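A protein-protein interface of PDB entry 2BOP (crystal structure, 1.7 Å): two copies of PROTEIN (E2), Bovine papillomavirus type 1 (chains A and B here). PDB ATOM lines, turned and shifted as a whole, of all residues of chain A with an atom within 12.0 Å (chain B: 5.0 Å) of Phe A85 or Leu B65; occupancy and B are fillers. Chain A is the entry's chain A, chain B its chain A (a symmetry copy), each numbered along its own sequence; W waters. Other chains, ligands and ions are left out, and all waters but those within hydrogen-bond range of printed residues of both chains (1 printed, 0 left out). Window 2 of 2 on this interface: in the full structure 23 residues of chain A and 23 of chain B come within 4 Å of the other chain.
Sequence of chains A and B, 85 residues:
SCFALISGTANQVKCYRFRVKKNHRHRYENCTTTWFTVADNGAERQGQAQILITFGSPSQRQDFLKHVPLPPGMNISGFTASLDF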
ATOM      1  N   SER A   1       1.678  16.397  25.133  1.00  0.00           N
ATOM      2  CA  SER A   1       1.363  17.749  24.865  1.00  0.00           C
ATOM      3  C   SER A   1       0.843  18.567  26.026  1.00  0.00           C
ATOM      4  O   SER A   1       1.689  19.375  26.466  1.00  0.00           O
ATOM      5  CB  SER A   1       1.496  18.344  23.560  1.00  0.00           C
ATOM      6  OG  SER A   1       0.292  18.493  22.676  1.00  0.00           O
ATOM      7  N   ALA A  81       4.159  20.768  26.258  1.00  0.00           N
ATOM      8  CA  ALA A  81       5.454  20.235  25.871  1.00  0.00           C
ATOM      9  C   ALA A  81       5.510  19.863  24.394  1.00  0.00           C
ATOM     10  O   ALA A  81       4.429  19.521  23.828  1.00  0.00           O
ATOM     11  CB  ALA A  81       5.819  19.106  26.790  1.00  0.00           C
ATOM     12  N   SER A  82       6.525  20.336  23.689  1.00  0.00           N
ATOM     13  CA  SER A  82       6.757  19.947  22.298  1.00  0.00           C
ATOM     14  C   SER A  82       7.812  18.841  22.205  1.00  0.00           C
ATOM     15  O   SER A  82       8.741  18.846  23.011  1.00  0.00           O
ATOM     16  CB  SER A  82       7.370  21.112  21.437  1.00  0.00           C
ATOM     17  OG  SER A  82       6.291  22.045  21.361  1.00  0.00           O
ATOM     18  N   LEU A  83       7.595  17.861  21.379  1.00  0.00           N
ATOM     19  CA  LEU A  83       8.599  16.824  21.109  1.00  0.00           C
ATOM     20  C   LEU A  83       9.765  17.431  20.313  1.00  0.00           C
ATOM     21  O   LEU A  83       9.535  18.018  19.217  1.00  0.00           O
ATOM     22  CB  LEU A  83       7.971  15.667  20.306  1.00  0.00           C
ATOM     23  CG  LEU A  83       8.887  14.452  20.116  1.00  0.00           C
ATOM     24  CD1 LEU A  83       8.823  13.499  21.306  1.00  0.00           C
ATOM     25  CD2 LEU A  83       8.490  13.615  18.891  1.00  0.00           C
ATOM     26  N   ASP A  84      10.957  17.233  20.778  1.00  0.00           N
ATOM     27  CA  ASP A  84      12.217  17.631  20.155  1.00  0.00           C
ATOM     28  C   ASP A  84      12.720  16.459  19.308  1.00  0.00           C
ATOM     29  O   ASP A  84      13.259  16.642  18.191  1.00  0.00           O
ATOM     30  CB  ASP A  84      13.297  18.103  21.186  1.00  0.00           C
ATOM     31  CG  ASP A  84      12.898  19.433  21.845  1.00  0.00           C
ATOM     32  OD1 ASP A  84      12.281  20.319  21.234  1.00  0.00           O
ATOM     33  OD2 ASP A  84      13.087  19.513  23.056  1.00  0.00           O
ATOM     34  N   PHE A  85      12.699  15.251  19.862  1.00  0.00           N
ATOM     35  CA  PHE A  85      13.131  14.036  19.171  1.00  0.00           C
ATOM     36  C   PHE A  85      12.577  12.824  19.847  1.00  0.00           C
ATOM     37  O   PHE A  85      12.626  11.691  19.197  1.00  0.00           O
ATOM     38  CB  PHE A  85      14.712  13.965  19.123  1.00  0.00           C
ATOM     39  CG  PHE A  85      15.383  13.986  20.457  1.00  0.00           C
ATOM     40  CD1 PHE A  85      15.573  12.862  21.212  1.00  0.00           C
ATOM     41  CD2 PHE A  85      15.842  15.283  20.930  1.00  0.00           C
ATOM     42  CE1 PHE A  85      16.219  12.965  22.461  1.00  0.00           C
ATOM     43  CE2 PHE A  85      16.497  15.342  22.207  1.00  0.00           C
ATOM     44  CZ  PHE A  85      16.531  14.205  23.011  1.00  0.00           C
ATOM     45  OXT PHE A  85      12.128  12.802  21.022  1.00  0.00           O
ATOM     46  N   ARG B  61      21.850  18.574  27.145  1.00  0.00           N
ATOM     47  CA  ARG B  61      21.070  17.448  26.683  1.00  0.00           C
ATOM     48  C   ARG B  61      21.829  16.788  25.546  1.00  0.00           C
ATOM     49  O   ARG B  61      21.863  15.553  25.407  1.00  0.00           O
ATOM     50  CB  ARG B  61      19.611  17.827  26.275  1.00  0.00           C
ATOM     51  CG  ARG B  61      18.784  16.619  25.862  1.00  0.00           C
ATOM     52  CD  ARG B  61      17.336  16.939  25.724  1.00  0.00           C
ATOM     53  NE  ARG B  61      17.134  17.945  24.685  1.00  0.00           N
ATOM     54  CZ  ARG B  61      15.888  18.344  24.300  1.00  0.00           C
ATOM     55  NH1 ARG B  61      14.835  17.971  24.991  1.00  0.00           N
ATOM     56  NH2 ARG B  61      15.827  19.275  23.409  1.00  0.00           N
ATOM     57  N   GLN B  62      22.315  17.619  24.621  1.00  0.00           N
ATOM     58  CA  GLN B  62      23.212  17.144  23.556  1.00  0.00           C
ATOM     59  C   GLN B  62      24.480  16.491  24.076  1.00  0.00           C
ATOM     60  O   GLN B  62      24.697  15.402  23.524  1.00  0.00           O
ATOM     61  CB  GLN B  62      23.619  18.304  22.635  1.00  0.00           C
ATOM     62  CG  GLN B  62      22.435  18.801  21.874  1.00  0.00           C
ATOM     63  CD  GLN B  62      22.813  20.014  21.061  1.00  0.00           C
ATOM     64  OE1 GLN B  62      22.976  21.127  21.626  1.00  0.00           O
ATOM     65  NE2 GLN B  62      23.271  19.733  19.819  1.00  0.00           N
ATOM     66  N   ASP B  63      25.095  16.958  25.089  1.00  0.00           N
ATOM     67  CA  ASP B  63      26.291  16.354  25.731  1.00  0.00           C
ATOM     68  C   ASP B  63      25.930  14.940  26.210  1.00  0.00           C
ATOM     69  O   ASP B  63      26.561  13.938  25.957  1.00  0.00           O
ATOM     70  CB  ASP B  63      26.826  17.158  26.924  1.00  0.00           C
ATOM     71  CG  ASP B  63      28.096  16.471  27.440  1.00  0.00           C
ATOM     72  OD1 ASP B  63      28.991  16.214  26.548  1.00  0.00           O
ATOM     73  OD2 ASP B  63      28.181  15.837  28.503  1.00  0.00           O
ATOM     74  N   PHE B  64      24.789  14.894  26.921  1.00  0.00           N
ATOM     75  CA  PHE B  64      24.183  13.634  27.385  1.00  0.00           C
ATOM     76  C   PHE B  64      23.962  12.681  26.268  1.00  0.00           C
ATOM     77  O   PHE B  64      24.314  11.480  26.471  1.00  0.00           O
ATOM     78  CB  PHE B  64      22.885  13.958  28.208  1.00  0.00           C
ATOM     79  CG  PHE B  64      22.359  12.736  28.974  1.00  0.00           C
ATOM     80  CD1 PHE B  64      21.473  11.874  28.359  1.00  0.00           C
ATOM     81  CD2 PHE B  64      22.523  12.720  30.364  1.00  0.00           C
ATOM     82  CE1 PHE B  64      20.958  10.802  29.113  1.00  0.00           C
ATOM     83  CE2 PHE B  64      22.121  11.605  31.086  1.00  0.00           C
ATOM     84  CZ  PHE B  64      21.243  10.696  30.454  1.00  0.00           C
ATOM     85  N   LEU B  65      23.269  12.998  25.192  1.00  0.00           N
ATOM     86  CA  LEU B  65      22.971  12.110  24.094  1.00  0.00           C
ATOM     87  C   LEU B  65      24.250  11.531  23.419  1.00  0.00           C
ATOM     88  O   LEU B  65      24.238  10.369  23.101  1.00  0.00           O
ATOM     89  CB  LEU B  65      22.209  12.988  23.078  1.00  0.00           C
ATOM     90  CG  LEU B  65      20.759  13.284  23.426  1.00  0.00           C
ATOM     91  CD1 LEU B  65      20.071  14.075  22.354  1.00  0.00           C
ATOM     92  CD2 LEU B  65      20.081  11.907  23.629  1.00  0.00           C
ATOM     93  N   LYS B  66      25.254  12.352  23.383  1.00  0.00           N
ATOM     94  CA  LYS B  66      26.560  11.957  22.772  1.00  0.00           C
ATOM     95  C   LYS B  66      27.408  11.090  23.662  1.00  0.00           C
ATOM     96  O   LYS B  66      27.879  10.001  23.155  1.00  0.00           O
ATOM     97  CB  LYS B  66      27.332  13.253  22.438  1.00  0.00           C
ATOM     98  CG  LYS B  66      26.716  13.853  21.099  1.00  0.00           C
ATOM     99  CD  LYS B  66      27.154  15.320  20.945  1.00  0.00           C
ATOM    100  CE  LYS B  66      26.596  15.715  19.519  1.00  0.00           C
ATOM    101  NZ  LYS B  66      25.100  15.257  19.627  1.00  0.00           N
ATOM    102  N   HIS B  67      27.368  11.226  24.968  1.00  0.00           N
ATOM    103  CA  HIS B  67      28.232  10.552  25.899  1.00  0.00           C
ATOM    104  C   HIS B  67      27.644   9.415  26.685  1.00  0.00           C
ATOM    105  O   HIS B  67      28.477   8.719  27.259  1.00  0.00           O
ATOM    106  CB  HIS B  67      28.932  11.527  26.899  1.00  0.00           C
ATOM    107  CG  HIS B  67      29.753  12.474  26.046  1.00  0.00           C
ATOM    108  ND1 HIS B  67      30.989  12.168  25.537  1.00  0.00           N
ATOM    109  CD2 HIS B  67      29.382  13.618  25.503  1.00  0.00           C
ATOM    110  CE1 HIS B  67      31.264  12.996  24.540  1.00  0.00           C
ATOM    111  NE2 HIS B  67      30.338  13.944  24.507  1.00  0.00           N
ATOM    112  N   VAL B  68      26.345   9.395  27.011  1.00  0.00           N
ATOM    113  CA  VAL B  68      25.807   8.349  27.887  1.00  0.00           C
ATOM    114  C   VAL B  68      25.252   7.254  26.978  1.00  0.00           C
ATOM    115  O   VAL B  68      24.338   7.540  26.200  1.00  0.00           O
ATOM    116  CB  VAL B  68      24.738   9.084  28.757  1.00  0.00           C
ATOM    117  CG1 VAL B  68      24.218   8.088  29.768  1.00  0.00           C
ATOM    118  CG2 VAL B  68      25.429  10.283  29.498  1.00  0.00           C
ATOM    119  N   ILE B  76      14.654   6.742  24.224  1.00  0.00           N
ATOM    120  CA  ILE B  76      14.734   8.116  24.781  1.00  0.00           C
ATOM    121  C   ILE B  76      13.923   9.093  23.908  1.00  0.00           C
ATOM    122  O   ILE B  76      14.004   8.966  22.676  1.00  0.00           O
ATOM    123  CB  ILE B  76      16.166   8.618  24.973  1.00  0.00           C
ATOM    124  CG1 ILE B  76      16.111  10.061  25.553  1.00  0.00           C
ATOM    125  CG2 ILE B  76      16.970   8.598  23.631  1.00  0.00           C
ATOM    126  CD1 ILE B  76      17.444  10.510  26.218  1.00  0.00           C
ATOM    127  N   SER B  77      13.161   9.961  24.491  1.00  0.00           N
ATOM    128  CA  SER B  77      12.465  11.014  23.700  1.00  0.00           C
ATOM    129  C   SER B  77      12.820  12.366  24.389  1.00  0.00           C
ATOM    130  O   SER B  77      12.778  12.336  25.663  1.00  0.00           O
ATOM    131  CB  SER B  77      10.930  10.918  23.764  1.00  0.00           C
ATOM    132  OG  SER B  77      10.572   9.740  23.049  1.00  0.00           O
ATOM    133  N   GLY B  78      12.920  13.409  23.647  1.00  0.00           N
ATOM    134  CA  GLY B  78      13.290  14.715  24.255  1.00  0.00           C
ATOM    135  C   GLY B  78      12.208  15.720  23.976  1.00  0.00           C
ATOM    136  O   GLY B  78      11.425  15.568  23.038  1.00  0.00           O
HETATM  137  O   HOH W   1      10.982   9.937  20.187  1.00  0.00           O
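The guanidinium group of Arg B61 is in salt-bridge range of the side-chain carboxylate of Asp A84.
The backbone NH (N) of Gly B78 lies within hydrogen-bond range of the chain-end carboxylate (OXT) of Phe A85 (2.8 Å).
The backbone carbonyl oxygen of Gly B78 sits at hydrogen-bond distance from the backbone NH of Asp A84 (2.8 Å).
Of the 11 printed residues of chain B, 4 touch a printed residue of chain A.
Hydrophobic or aromatic side chains of chain A within 4 Å of the printed part of chain B: Leu A83 and Phe A85.
Water W1 lies within hydrogen-bond range of the chain-end carboxylate (O) of Phe A85 (2.6 Å) and the side-chain hydroxyl (OG) of Ser B77 (2.9 Å).
Of chain B, only Arg B61, Leu B65, Ser B77 and Gly B78 come within 4 Å of Phe A85.
No residue of chain A comes within 4 Å of Phe B64.
No residue of chain A comes within 4 Å of Lys B66.
No residue of chain A comes within 4 Å of Val B68.
Of chain A, only Phe A85 (3.2 Å) comes within 4 Å of Ser B77.
Of chain A, only Leu A83, Asp A84 and Phe A85 come within 4 Å of Gly B78.
Of the printed residues of chain B, Asp A84 touches Arg B61 and Gly B78.
Of the printed residues of chain B, Leu A83 touches Gly B78.
The nearest residue of chain B that does not touch Phe A85 is Ile B76 (4.2 Å).
No position is printed for both chains.
Of the 7 pairs that touch across the chains among the printed residues, none has its exchanged pair printed and touching as well.
Leu A83 touches Gly B78 (CA to O, 3.6 Å).
Phe A85 touches Arg B61.
CD1 of Leu B65 touches CZ of Phe A85, at 3.6 Å.
Phe A85 touches Ser B77 (OXT to CA, 3.2 Å).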
